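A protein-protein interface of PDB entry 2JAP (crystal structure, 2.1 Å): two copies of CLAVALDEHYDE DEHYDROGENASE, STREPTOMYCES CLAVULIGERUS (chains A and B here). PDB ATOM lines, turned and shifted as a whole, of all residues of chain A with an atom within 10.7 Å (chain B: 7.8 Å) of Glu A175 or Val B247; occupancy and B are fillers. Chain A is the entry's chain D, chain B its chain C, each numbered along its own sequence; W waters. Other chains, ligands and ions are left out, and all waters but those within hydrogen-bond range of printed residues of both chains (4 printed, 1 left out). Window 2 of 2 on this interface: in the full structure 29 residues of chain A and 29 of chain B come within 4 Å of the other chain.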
ATOM      1  N   LEU A 127     -12.736  -5.589  33.992  1.00  0.00           N
ATOM      2  CA  LEU A 127     -12.676  -4.175  33.592  1.00  0.00           C
ATOM      3  C   LEU A 127     -11.270  -3.588  33.370  1.00  0.00           C
ATOM      4  O   LEU A 127     -11.026  -2.985  32.323  1.00  0.00           O
ATOM      5  CB  LEU A 127     -13.506  -3.306  34.554  1.00  0.00           C
ATOM      6  CG  LEU A 127     -14.250  -2.092  33.993  1.00  0.00           C
ATOM      7  CD1 LEU A 127     -14.948  -2.410  32.682  1.00  0.00           C
ATOM      8  CD2 LEU A 127     -15.246  -1.554  35.023  1.00  0.00           C
ATOM      9  N   LEU A 130     -10.123  -4.982  30.090  1.00  0.00           N
ATOM     10  CA  LEU A 130     -10.910  -4.503  28.957  1.00  0.00           C
ATOM     11  C   LEU A 130     -10.584  -3.051  28.647  1.00  0.00           C
ATOM     12  O   LEU A 130     -10.576  -2.651  27.484  1.00  0.00           O
ATOM     13  CB  LEU A 130     -12.408  -4.666  29.207  1.00  0.00           C
ATOM     14  CG  LEU A 130     -12.937  -6.084  29.414  1.00  0.00           C
ATOM     15  CD1 LEU A 130     -14.374  -6.038  29.941  1.00  0.00           C
ATOM     16  CD2 LEU A 130     -12.856  -6.909  28.126  1.00  0.00           C
ATOM     17  N   LEU A 131     -10.317  -2.266  29.689  1.00  0.00           N
ATOM     18  CA  LEU A 131      -9.931  -0.870  29.516  1.00  0.00           C
ATOM     19  C   LEU A 131      -8.633  -0.731  28.715  1.00  0.00           C
ATOM     20  O   LEU A 131      -8.537   0.143  27.848  1.00  0.00           O
ATOM     21  CB  LEU A 131      -9.817  -0.161  30.870  1.00  0.00           C
ATOM     22  CG  LEU A 131     -11.133   0.265  31.540  1.00  0.00           C
ATOM     23  CD1 LEU A 131     -10.921   0.465  33.034  1.00  0.00           C
ATOM     24  CD2 LEU A 131     -11.695   1.528  30.907  1.00  0.00           C
ATOM     25  N   LYS A 134      -9.360  -1.873  25.033  1.00  0.00           N
ATOM     26  CA  LYS A 134     -10.547  -1.237  24.447  1.00  0.00           C
ATOM     27  C   LYS A 134     -11.541  -2.327  24.013  1.00  0.00           C
ATOM     28  O   LYS A 134     -12.056  -2.328  22.884  1.00  0.00           O
ATOM     29  CB  LYS A 134     -10.161  -0.321  23.265  1.00  0.00           C
ATOM     30  CG  LYS A 134      -9.028   0.684  23.554  1.00  0.00           C
ATOM     31  CD  LYS A 134      -9.345   1.570  24.761  1.00  0.00           C
ATOM     32  CE  LYS A 134      -8.279   2.631  25.022  1.00  0.00           C
ATOM     33  NZ  LYS A 134      -8.693   3.501  26.188  1.00  0.00           N
ATOM     34  N   GLY A 135     -11.781  -3.269  24.922  1.00  0.00           N
ATOM     35  CA  GLY A 135     -12.546  -4.466  24.611  1.00  0.00           C
ATOM     36  C   GLY A 135     -14.050  -4.322  24.759  1.00  0.00           C
ATOM     37  O   GLY A 135     -14.584  -3.218  24.889  1.00  0.00           O
ATOM     38  N   SER A 166     -25.779  -2.483  33.273  1.00  0.00           N
ATOM     39  CA  SER A 166     -25.031  -2.435  32.017  1.00  0.00           C
ATOM     40  C   SER A 166     -25.118  -1.090  31.294  1.00  0.00           C
ATOM     41  O   SER A 166     -24.114  -0.614  30.751  1.00  0.00           O
ATOM     42  CB  SER A 166     -25.495  -3.560  31.096  1.00  0.00           C
ATOM     43  OG  SER A 166     -25.348  -4.809  31.757  1.00  0.00           O
ATOM     44  N   GLU A 167     -26.307  -0.485  31.275  1.00  0.00           N
ATOM     45  CA  GLU A 167     -26.458   0.872  30.747  1.00  0.00           C
ATOM     46  C   GLU A 167     -25.617   1.855  31.556  1.00  0.00           C
ATOM     47  O   GLU A 167     -24.924   2.703  30.994  1.00  0.00           O
ATOM     48  CB  GLU A 167     -27.933   1.315  30.729  1.00  0.00           C
ATOM     49  CG  GLU A 167     -28.166   2.836  30.565  1.00  0.00           C
ATOM     50  CD  GLU A 167     -27.441   3.465  29.365  1.00  0.00           C
ATOM     51  OE1 GLU A 167     -27.087   2.749  28.397  1.00  0.00           O
ATOM     52  OE2 GLU A 167     -27.236   4.692  29.391  1.00  0.00           O
ATOM     53  N   THR A 168     -25.677   1.739  32.876  1.00  0.00           N
ATOM     54  CA  THR A 168     -24.865   2.597  33.743  1.00  0.00           C
ATOM     55  C   THR A 168     -23.380   2.389  33.473  1.00  0.00           C
ATOM     56  O   THR A 168     -22.635   3.360  33.333  1.00  0.00           O
ATOM     57  CB  THR A 168     -25.145   2.366  35.227  1.00  0.00           C
ATOM     58  OG1 THR A 168     -26.558   2.348  35.452  1.00  0.00           O
ATOM     59  CG2 THR A 168     -24.499   3.479  36.082  1.00  0.00           C
ATOM     60  N   LEU A 169     -22.964   1.126  33.405  1.00  0.00           N
ATOM     61  CA  LEU A 169     -21.594   0.775  33.031  1.00  0.00           C
ATOM     62  C   LEU A 169     -21.177   1.433  31.713  1.00  0.00           C
ATOM     63  O   LEU A 169     -20.096   2.018  31.634  1.00  0.00           O
ATOM     64  CB  LEU A 169     -21.409  -0.750  32.952  1.00  0.00           C
ATOM     65  CG  LEU A 169     -20.031  -1.262  32.514  1.00  0.00           C
ATOM     66  CD1 LEU A 169     -18.948  -0.961  33.561  1.00  0.00           C
ATOM     67  CD2 LEU A 169     -20.098  -2.743  32.217  1.00  0.00           C
ATOM     68  N   ARG A 170     -22.031   1.343  30.695  1.00  0.00           N
ATOM     69  CA  ARG A 170     -21.779   1.987  29.399  1.00  0.00           C
ATOM     70  C   ARG A 170     -21.468   3.465  29.589  1.00  0.00           C
ATOM     71  O   ARG A 170     -20.463   3.950  29.089  1.00  0.00           O
ATOM     72  CB  ARG A 170     -22.966   1.796  28.439  1.00  0.00           C
ATOM     73  CG  ARG A 170     -22.680   2.109  26.975  1.00  0.00           C
ATOM     74  CD  ARG A 170     -23.978   2.387  26.162  1.00  0.00           C
ATOM     75  NE  ARG A 170     -24.807   3.437  26.783  1.00  0.00           N
ATOM     76  CZ  ARG A 170     -24.591   4.750  26.669  1.00  0.00           C
ATOM     77  NH1 ARG A 170     -23.587   5.213  25.930  1.00  0.00           N
ATOM     78  NH2 ARG A 170     -25.385   5.605  27.288  1.00  0.00           N
ATOM     79  N   GLN A 171     -22.316   4.174  30.327  1.00  0.00           N
ATOM     80  CA  GLN A 171     -22.083   5.591  30.601  1.00  0.00           C
ATOM     81  C   GLN A 171     -20.711   5.830  31.241  1.00  0.00           C
ATOM     82  O   GLN A 171     -20.036   6.810  30.914  1.00  0.00           O
ATOM     83  CB  GLN A 171     -23.188   6.157  31.497  1.00  0.00           C
ATOM     84  CG  GLN A 171     -24.538   6.280  30.792  1.00  0.00           C
ATOM     85  CD  GLN A 171     -25.609   6.879  31.690  1.00  0.00           C
ATOM     86  OE1 GLN A 171     -25.311   7.712  32.540  1.00  0.00           O
ATOM     87  NE2 GLN A 171     -26.867   6.441  31.507  1.00  0.00           N
ATOM     88  N   GLU A 172     -20.312   4.923  32.136  1.00  0.00           N
ATOM     89  CA  GLU A 172     -19.067   5.049  32.898  1.00  0.00           C
ATOM     90  C   GLU A 172     -17.787   4.754  32.100  1.00  0.00           C
ATOM     91  O   GLU A 172     -16.749   5.357  32.363  1.00  0.00           O
ATOM     92  CB  GLU A 172     -19.111   4.169  34.163  1.00  0.00           C
ATOM     93  CG  GLU A 172     -20.032   4.687  35.289  1.00  0.00           C
ATOM     94  CD  GLU A 172     -20.097   3.760  36.512  1.00  0.00           C
ATOM     95  OE1 GLU A 172     -19.165   2.950  36.726  1.00  0.00           O
ATOM     96  OE2 GLU A 172     -21.086   3.856  37.284  1.00  0.00           O
ATOM     97  N   VAL A 173     -17.857   3.833  31.139  1.00  0.00           N
ATOM     98  CA  VAL A 173     -16.640   3.317  30.478  1.00  0.00           C
ATOM     99  C   VAL A 173     -16.581   3.508  28.959  1.00  0.00           C
ATOM    100  O   VAL A 173     -15.523   3.334  28.353  1.00  0.00           O
ATOM    101  CB  VAL A 173     -16.397   1.814  30.810  1.00  0.00           C
ATOM    102  CG1 VAL A 173     -16.345   1.601  32.314  1.00  0.00           C
ATOM    103  CG2 VAL A 173     -17.475   0.920  30.158  1.00  0.00           C
ATOM    104  N   THR A 174     -17.710   3.862  28.350  1.00  0.00           N
ATOM    105  CA  THR A 174     -17.794   3.957  26.893  1.00  0.00           C
ATOM    106  C   THR A 174     -16.783   4.931  26.282  1.00  0.00           C
ATOM    107  O   THR A 174     -16.186   4.636  25.246  1.00  0.00           O
ATOM    108  CB  THR A 174     -19.252   4.222  26.397  1.00  0.00           C
ATOM    109  OG1 THR A 174     -19.421   3.695  25.077  1.00  0.00           O
ATOM    110  CG2 THR A 174     -19.626   5.706  26.422  1.00  0.00           C
ATOM    111  N   GLU A 175     -16.568   6.063  26.944  1.00  0.00           N
ATOM    112  CA  GLU A 175     -15.646   7.085  26.455  1.00  0.00           C
ATOM    113  C   GLU A 175     -14.180   6.633  26.443  1.00  0.00           C
ATOM    114  O   GLU A 175     -13.367   7.198  25.716  1.00  0.00           O
ATOM    115  CB  GLU A 175     -15.792   8.364  27.268  1.00  0.00           C
ATOM    116  CG  GLU A 175     -17.057   9.121  26.976  1.00  0.00           C
ATOM    117  CD  GLU A 175     -17.341  10.160  28.027  1.00  0.00           C
ATOM    118  OE1 GLU A 175     -17.271   9.831  29.231  1.00  0.00           O
ATOM    119  OE2 GLU A 175     -17.635  11.310  27.652  1.00  0.00           O
ATOM    120  N   ARG A 176     -13.863   5.621  27.251  1.00  0.00           N
ATOM    121  CA  ARG A 176     -12.545   4.997  27.261  1.00  0.00           C
ATOM    122  C   ARG A 176     -12.490   3.773  26.348  1.00  0.00           C
ATOM    123  O   ARG A 176     -11.527   3.013  26.385  1.00  0.00           O
ATOM    124  CB  ARG A 176     -12.121   4.623  28.687  1.00  0.00           C
ATOM    125  CG  ARG A 176     -11.679   5.805  29.537  1.00  0.00           C
ATOM    126  CD  ARG A 176     -11.477   5.394  30.990  1.00  0.00           C
ATOM    127  NE  ARG A 176     -12.748   5.105  31.642  1.00  0.00           N
ATOM    128  CZ  ARG A 176     -12.883   4.632  32.877  1.00  0.00           C
ATOM    129  NH1 ARG A 176     -11.819   4.380  33.633  1.00  0.00           N
ATOM    130  NH2 ARG A 176     -14.102   4.414  33.360  1.00  0.00           N
ATOM    131  N   GLY A 177     -13.534   3.580  25.543  1.00  0.00           N
ATOM    132  CA  GLY A 177     -13.512   2.586  24.477  1.00  0.00           C
ATOM    133  C   GLY A 177     -13.855   1.163  24.870  1.00  0.00           C
ATOM    134  O   GLY A 177     -13.574   0.226  24.117  1.00  0.00           O
ATOM    135  N   VAL A 178     -14.452   0.995  26.048  1.00  0.00           N
ATOM    136  CA  VAL A 178     -15.009  -0.299  26.430  1.00  0.00           C
ATOM    137  C   VAL A 178     -16.461  -0.339  25.992  1.00  0.00           C
ATOM    138  O   VAL A 178     -17.283   0.467  26.447  1.00  0.00           O
ATOM    139  CB  VAL A 178     -14.891  -0.585  27.944  1.00  0.00           C
ATOM    140  CG1 VAL A 178     -15.489  -1.942  28.273  1.00  0.00           C
ATOM    141  CG2 VAL A 178     -13.437  -0.551  28.375  1.00  0.00           C
ATOM    142  N   ARG A 179     -16.771  -1.272  25.095  1.00  0.00           N
ATOM    143  CA  ARG A 179     -18.112  -1.383  24.540  1.00  0.00           C
ATOM    144  C   ARG A 179     -18.966  -2.292  25.410  1.00  0.00           C
ATOM    145  O   ARG A 179     -18.526  -3.366  25.817  1.00  0.00           O
ATOM    146  CB  ARG A 179     -18.080  -1.902  23.098  1.00  0.00           C
ATOM    147  CG  ARG A 179     -17.195  -1.085  22.160  1.00  0.00           C
ATOM    148  CD  ARG A 179     -17.383  -1.490  20.716  1.00  0.00           C
ATOM    149  NE  ARG A 179     -16.996  -2.879  20.505  1.00  0.00           N
ATOM    150  CZ  ARG A 179     -17.066  -3.517  19.342  1.00  0.00           C
ATOM    151  NH1 ARG A 179     -17.518  -2.898  18.248  1.00  0.00           N
ATOM    152  NH2 ARG A 179     -16.685  -4.784  19.279  1.00  0.00           N
ATOM    153  N   VAL A 180     -20.184  -1.844  25.697  1.00  0.00           N
ATOM    154  CA  VAL A 180     -21.131  -2.630  26.475  1.00  0.00           C
ATOM    155  C   VAL A 180     -22.293  -3.076  25.591  1.00  0.00           C
ATOM    156  O   VAL A 180     -23.072  -2.255  25.086  1.00  0.00           O
ATOM    157  CB  VAL A 180     -21.647  -1.859  27.707  1.00  0.00           C
ATOM    158  CG1 VAL A 180     -22.638  -2.716  28.502  1.00  0.00           C
ATOM    159  CG2 VAL A 180     -20.463  -1.441  28.591  1.00  0.00           C
ATOM    160  N   HIS A 232     -15.169  -0.675  16.046  1.00  0.00           N
ATOM    161  CA  HIS A 232     -15.047  -0.202  17.436  1.00  0.00           C
ATOM    162  C   HIS A 232     -15.867   1.055  17.752  1.00  0.00           C
ATOM    163  O   HIS A 232     -16.346   1.208  18.874  1.00  0.00           O
ATOM    164  CB  HIS A 232     -13.578  -0.031  17.877  1.00  0.00           C
ATOM    165  CG  HIS A 232     -13.443   0.433  19.300  1.00  0.00           C
ATOM    166  ND1 HIS A 232     -13.309   1.764  19.641  1.00  0.00           N
ATOM    167  CD2 HIS A 232     -13.497  -0.249  20.469  1.00  0.00           C
ATOM    168  CE1 HIS A 232     -13.247   1.875  20.956  1.00  0.00           C
ATOM    169  NE2 HIS A 232     -13.359   0.670  21.483  1.00  0.00           N
ATOM    170  N   HIS A 233     -16.042   1.931  16.764  1.00  0.00           N
ATOM    171  CA  HIS A 233     -16.823   3.169  16.917  1.00  0.00           C
ATOM    172  C   HIS A 233     -18.339   2.924  17.120  1.00  0.00           C
ATOM    173  O   HIS A 233     -19.100   3.845  17.441  1.00  0.00           O
ATOM    174  CB  HIS A 233     -16.566   4.105  15.720  1.00  0.00           C
ATOM    175  CG  HIS A 233     -17.145   3.616  14.426  1.00  0.00           C
ATOM    176  ND1 HIS A 233     -16.400   2.957  13.472  1.00  0.00           N
ATOM    177  CD2 HIS A 233     -18.405   3.685  13.935  1.00  0.00           C
ATOM    178  CE1 HIS A 233     -17.172   2.653  12.444  1.00  0.00           C
ATOM    179  NE2 HIS A 233     -18.396   3.076  12.704  1.00  0.00           N
ATOM    180  N   THR A 235     -21.188   0.743  19.187  1.00  0.00           N
ATOM    181  CA  THR A 235     -21.583  -0.147  20.254  1.00  0.00           C
ATOM    182  C   THR A 235     -23.015  -0.625  20.014  1.00  0.00           C
ATOM    183  O   THR A 235     -23.963   0.158  20.098  1.00  0.00           O
ATOM    184  CB  THR A 235     -21.475   0.504  21.640  1.00  0.00           C
ATOM    185  OG1 THR A 235     -20.109   0.804  21.905  1.00  0.00           O
ATOM    186  CG2 THR A 235     -21.989  -0.464  22.735  1.00  0.00           C
ATOM    187  N   HIS A 237     -25.561  -1.766  21.591  1.00  0.00           N
ATOM    188  CA  HIS A 237     -25.859  -1.827  23.002  1.00  0.00           C
ATOM    189  C   HIS A 237     -26.963  -2.828  23.346  1.00  0.00           C
ATOM    190  O   HIS A 237     -26.927  -3.432  24.407  1.00  0.00           O
ATOM    191  CB  HIS A 237     -26.170  -0.447  23.574  1.00  0.00           C
ATOM    192  CG  HIS A 237     -26.412  -0.470  25.051  1.00  0.00           C
ATOM    193  ND1 HIS A 237     -25.456  -0.886  25.949  1.00  0.00           N
ATOM    194  CD2 HIS A 237     -27.514  -0.184  25.780  1.00  0.00           C
ATOM    195  CE1 HIS A 237     -25.949  -0.833  27.173  1.00  0.00           C
ATOM    196  NE2 HIS A 237     -27.203  -0.421  27.097  1.00  0.00           N
ATOM    197  N   ILE B 143     -32.227   6.226  18.385  1.00  0.00           N
ATOM    198  CA  ILE B 143     -31.980   6.462  19.807  1.00  0.00           C
ATOM    199  C   ILE B 143     -33.088   7.368  20.367  1.00  0.00           C
ATOM    200  O   ILE B 143     -33.455   7.264  21.535  1.00  0.00           O
ATOM    201  CB  ILE B 143     -30.563   7.086  20.038  1.00  0.00           C
ATOM    202  CG1 ILE B 143     -30.258   7.226  21.533  1.00  0.00           C
ATOM    203  CG2 ILE B 143     -30.413   8.429  19.294  1.00  0.00           C
ATOM    204  CD1 ILE B 143     -28.818   7.572  21.871  1.00  0.00           C
ATOM    205  N   VAL B 147     -34.558   7.205  24.112  1.00  0.00           N
ATOM    206  CA  VAL B 147     -34.114   8.177  25.109  1.00  0.00           C
ATOM    207  C   VAL B 147     -34.525   9.584  24.682  1.00  0.00           C
ATOM    208  O   VAL B 147     -34.523   9.901  23.495  1.00  0.00           O
ATOM    209  CB  VAL B 147     -32.575   8.115  25.394  1.00  0.00           C
ATOM    210  CG1 VAL B 147     -32.190   6.828  26.150  1.00  0.00           C
ATOM    211  CG2 VAL B 147     -31.771   8.217  24.137  1.00  0.00           C
ATOM    212  N   VAL B 149     -33.806  13.663  24.882  1.00  0.00           N
ATOM    213  CA  VAL B 149     -32.934  14.803  25.194  1.00  0.00           C
ATOM    214  C   VAL B 149     -33.638  16.112  24.791  1.00  0.00           C
ATOM    215  O   VAL B 149     -34.577  16.084  23.986  1.00  0.00           O
ATOM    216  CB  VAL B 149     -31.530  14.722  24.475  1.00  0.00           C
ATOM    217  CG1 VAL B 149     -30.735  13.491  24.939  1.00  0.00           C
ATOM    218  CG2 VAL B 149     -31.679  14.741  22.948  1.00  0.00           C
ATOM    219  N   ARG B 208     -22.295  19.441  19.532  1.00  0.00           N
ATOM    220  CA  ARG B 208     -22.400  18.301  20.434  1.00  0.00           C
ATOM    221  C   ARG B 208     -21.868  17.012  19.795  1.00  0.00           C
ATOM    222  O   ARG B 208     -21.204  16.219  20.469  1.00  0.00           O
ATOM    223  CB  ARG B 208     -23.825  18.131  20.945  1.00  0.00           C
ATOM    224  CG  ARG B 208     -24.047  16.860  21.751  1.00  0.00           C
ATOM    225  CD  ARG B 208     -25.482  16.421  21.606  1.00  0.00           C
ATOM    226  NE  ARG B 208     -25.672  14.988  21.841  1.00  0.00           N
ATOM    227  CZ  ARG B 208     -26.845  14.369  21.728  1.00  0.00           C
ATOM    228  NH1 ARG B 208     -27.930  15.058  21.374  1.00  0.00           N
ATOM    229  NH2 ARG B 208     -26.938  13.064  21.965  1.00  0.00           N
ATOM    230  N   ILE B 212     -17.295  13.193  18.578  1.00  0.00           N
ATOM    231  CA  ILE B 212     -17.441  11.743  18.585  1.00  0.00           C
ATOM    232  C   ILE B 212     -17.176  11.155  17.200  1.00  0.00           C
ATOM    233  O   ILE B 212     -17.406  11.816  16.186  1.00  0.00           O
ATOM    234  CB  ILE B 212     -18.872  11.291  19.076  1.00  0.00           C
ATOM    235  CG1 ILE B 212     -19.972  11.871  18.181  1.00  0.00           C
ATOM    236  CG2 ILE B 212     -19.110  11.686  20.545  1.00  0.00           C
ATOM    237  CD1 ILE B 212     -21.279  11.091  18.183  1.00  0.00           C
ATOM    238  N   ARG B 213     -16.690   9.918  17.166  1.00  0.00           N
ATOM    239  CA  ARG B 213     -16.717   9.152  15.931  1.00  0.00           C
ATOM    240  C   ARG B 213     -18.176   8.734  15.739  1.00  0.00           C
ATOM    241  O   ARG B 213     -18.749   7.994  16.554  1.00  0.00           O
ATOM    242  CB  ARG B 213     -15.768   7.956  15.989  1.00  0.00           C
ATOM    243  CG  ARG B 213     -14.307   8.326  16.150  1.00  0.00           C
ATOM    244  CD  ARG B 213     -13.476   7.124  16.615  1.00  0.00           C
ATOM    245  NE  ARG B 213     -14.062   6.498  17.801  1.00  0.00           N
ATOM    246  CZ  ARG B 213     -13.816   5.256  18.217  1.00  0.00           C
ATOM    247  NH1 ARG B 213     -12.982   4.465  17.547  1.00  0.00           N
ATOM    248  NH2 ARG B 213     -14.421   4.802  19.311  1.00  0.00           N
ATOM    249  N   ARG B 242     -25.274   2.401  19.264  1.00  0.00           N
ATOM    250  CA  ARG B 242     -24.808   3.708  19.732  1.00  0.00           C
ATOM    251  C   ARG B 242     -23.359   3.957  19.312  1.00  0.00           C
ATOM    252  O   ARG B 242     -22.584   3.008  19.178  1.00  0.00           O
ATOM    253  CB  ARG B 242     -24.850   3.774  21.263  1.00  0.00           C
ATOM    254  CG  ARG B 242     -26.213   3.798  21.914  1.00  0.00           C
ATOM    255  CD  ARG B 242     -25.964   3.938  23.398  1.00  0.00           C
ATOM    256  NE  ARG B 242     -27.158   4.062  24.212  1.00  0.00           N
ATOM    257  CZ  ARG B 242     -27.569   5.176  24.810  1.00  0.00           C
ATOM    258  NH1 ARG B 242     -26.916   6.314  24.672  1.00  0.00           N
ATOM    259  NH2 ARG B 242     -28.667   5.146  25.541  1.00  0.00           N
ATOM    260  N   PRO B 243     -22.981   5.238  19.129  1.00  0.00           N
ATOM    261  CA  PRO B 243     -21.555   5.535  18.972  1.00  0.00           C
ATOM    262  C   PRO B 243     -20.879   5.217  20.293  1.00  0.00           C
ATOM    263  O   PRO B 243     -21.365   5.641  21.348  1.00  0.00           O
ATOM    264  CB  PRO B 243     -21.528   7.049  18.717  1.00  0.00           C
ATOM    265  CG  PRO B 243     -22.936   7.428  18.366  1.00  0.00           C
ATOM    266  CD  PRO B 243     -23.804   6.462  19.097  1.00  0.00           C
ATOM    267  N   THR B 244     -19.805   4.440  20.238  1.00  0.00           N
ATOM    268  CA  THR B 244     -19.010   4.096  21.418  1.00  0.00           C
ATOM    269  C   THR B 244     -18.494   5.339  22.164  1.00  0.00           C
ATOM    270  O   THR B 244     -18.295   5.313  23.385  1.00  0.00           O
ATOM    271  CB  THR B 244     -17.838   3.188  20.992  1.00  0.00           C
ATOM    272  OG1 THR B 244     -18.368   2.066  20.277  1.00  0.00           O
ATOM    273  CG2 THR B 244     -17.026   2.687  22.181  1.00  0.00           C
ATOM    274  N   ASP B 245     -18.285   6.427  21.432  1.00  0.00           N
ATOM    275  CA  ASP B 245     -17.675   7.635  21.995  1.00  0.00           C
ATOM    276  C   ASP B 245     -18.673   8.470  22.781  1.00  0.00           C
ATOM    277  O   ASP B 245     -18.293   9.393  23.498  1.00  0.00           O
ATOM    278  CB  ASP B 245     -17.112   8.491  20.874  1.00  0.00           C
ATOM    279  CG  ASP B 245     -15.883   7.888  20.244  1.00  0.00           C
ATOM    280  OD1 ASP B 245     -15.278   6.968  20.839  1.00  0.00           O
ATOM    281  OD2 ASP B 245     -15.510   8.365  19.160  1.00  0.00           O
ATOM    282  N   GLN B 246     -19.951   8.139  22.637  1.00  0.00           N
ATOM    283  CA  GLN B 246     -21.029   8.980  23.143  1.00  0.00           C
ATOM    284  C   GLN B 246     -21.742   8.425  24.390  1.00  0.00           C
ATOM    285  O   GLN B 246     -22.434   7.403  24.326  1.00  0.00           O
ATOM    286  CB  GLN B 246     -22.044   9.230  22.029  1.00  0.00           C
ATOM    287  CG  GLN B 246     -23.142  10.205  22.369  1.00  0.00           C
ATOM    288  CD  GLN B 246     -24.244  10.150  21.341  1.00  0.00           C
ATOM    289  OE1 GLN B 246     -25.043   9.213  21.334  1.00  0.00           O
ATOM    290  NE2 GLN B 246     -24.281  11.135  20.447  1.00  0.00           N
ATOM    291  N   VAL B 247     -21.588   9.126  25.513  1.00  0.00           N
ATOM    292  CA  VAL B 247     -22.363   8.818  26.726  1.00  0.00           C
ATOM    293  C   VAL B 247     -23.853   9.055  26.453  1.00  0.00           C
ATOM    294  O   VAL B 247     -24.722   8.251  26.817  1.00  0.00           O
ATOM    295  CB  VAL B 247     -21.894   9.649  27.960  1.00  0.00           C
ATOM    296  CG1 VAL B 247     -22.751   9.350  29.193  1.00  0.00           C
ATOM    297  CG2 VAL B 247     -20.455   9.356  28.285  1.00  0.00           C
ATOM    298  OXT VAL B 247     -24.253  10.047  25.837  1.00  0.00           O
HETATM  299  O   HOH W   1     -29.074   2.663  26.528  1.00  0.00           O
HETATM  300  O   HOH W   2     -21.891   4.010  23.679  1.00  0.00           O
HETATM  301  O   HOH W   3     -28.982   6.341  28.057  1.00  0.00           O
HETATM  302  O   HOH W   4     -18.043   6.258  18.524  1.00  0.00           O
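OE1 of Glu A167 lies within salt-bridge range of NE of Arg A170 (2.9 Å). A ring nitrogen (NE2) of His A232 is in hydrogen-bond range of the backbone carbonyl oxygen (O) of Gly A177. N of Arg A179 sits at hydrogen-bond distance from O of Gly A135. The guanidinium group (NE) of Arg B213 lies within salt-bridge range of the side-chain carboxylate (OD2) of Asp B245 (2.7 Å). The chain-end carboxylate (O) of Val B247 lies within salt-bridge range of the guanidinium group (NH1) of Arg B242. NE2 of Gln A171 lies within hydrogen-bond range of OE2 of Glu A167, at 2.8 Å.
No position is printed for both chains.
Printed residues of chain B that touch a printed residue of chain A: Arg B213, Arg B242, Pro B243, Thr B244, Asp B245, Gln B246 and Val B247. Hydrophobic or aromatic side chains of chain B within 4 Å of the printed part of chain A: Val B247. Along chain B the printed residues that touch a printed residue of chain A span positions 213 to 247. Among the printed residues, 17 pairs touch across the chains. Among the printed residues, no Asp or Glu carboxylate lies within 4 Å of a Lys or Arg side-chain nitrogen of the other chain.
Water W1 bridges the guanidinium group (NH2) of Arg B242 (2.7 Å) and the side-chain carboxylate (OE1) of Glu A167 (2.7 Å). Water W4 lies within hydrogen-bond range of the backbone carbonyl oxygen of Arg B213 (2.7 Å), the backbone carbonyl oxygen of His A233 (2.8 Å), the backbone NH of Asp B245 (2.9 Å) and the backbone NH of Thr B244 (3.1 Å). Water W3 bridges OE2 of Glu A167 (2.7 Å) and NH2 of Arg B242 (2.8 Å). Water W2 lies within hydrogen-bond range of OG1 of Thr A174 (2.9 Å), O of Pro B243 (2.9 Å), NH1 of Arg A170 (3.1 Å) and O of Gln B246 (3.5 Å).
Ser A166 touches none of the printed residues of chain B. Thr A168 touches none of the printed residues of chain B. Of chain B, only Asp B245 and Val B247 come within 4 Å of Glu A175. Printed residues of chain A within 4 Å of Arg B242: Arg A170, His A233 and Thr A235. Of the printed residues of chain A, Pro B243 touches His A233 (3.4 Å). Gln B246 touches two residues of chain A. Of chain A, only Arg A170, Gln A171 and Glu A175 come within 4 Å of Val B247. The nearest residue of chain B that does not touch Glu A175 is Thr B244 (4.03 Å). The nearest printed residue of chain B that does not touch His A232 is Asp B245 (5.5 Å).
CG2 of Val B247 touches O of Gln A171, at 3.7 Å. Thr A174 touches Gln B246 (CG2 to O, 3.9 Å). Asp B245 touches Glu A175. Glu A175 touches Val B247 (CD to CG2, 3.2 Å). Thr B244 touches Arg A179. His A233 touches Arg B213. Arg B242 touches His A233. His A233 touches Pro B243.
The guanidinium group (NH2) of Arg A170 sits close to the guanidinium group (NH1) of Arg B242 (3.1 Å). The chain-end carboxylate (O) of Val B247 is in salt-bridge range of the guanidinium group (NH2) of Arg A170 (2.8 Å). The side-chain hydroxyl (OG1) of Thr A174 lies within hydrogen-bond range of the backbone carbonyl oxygen (O) of Thr B244. OG1 of Thr A235 sits at hydrogen-bond distance from OG1 of Thr B244 (2.7 Å). The backbone carbonyl oxygen (O) of Gln B246 lies within hydrogen-bond range of the guanidinium group (NH1) of Arg A170. OG1 of Thr B244 sits at hydrogen-bond distance from O of His A232. The guanidinium group (NH2) of Arg B213 lies within hydrogen-bond range of a ring nitrogen (ND1) of His A232. N of Thr A235 sits at hydrogen-bond distance from O of Arg B242 (2.7 Å). The backbone NH (N) of Thr B244 is in hydrogen-bond range of the backbone carbonyl oxygen (O) of His A233, at 2.9 Å.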
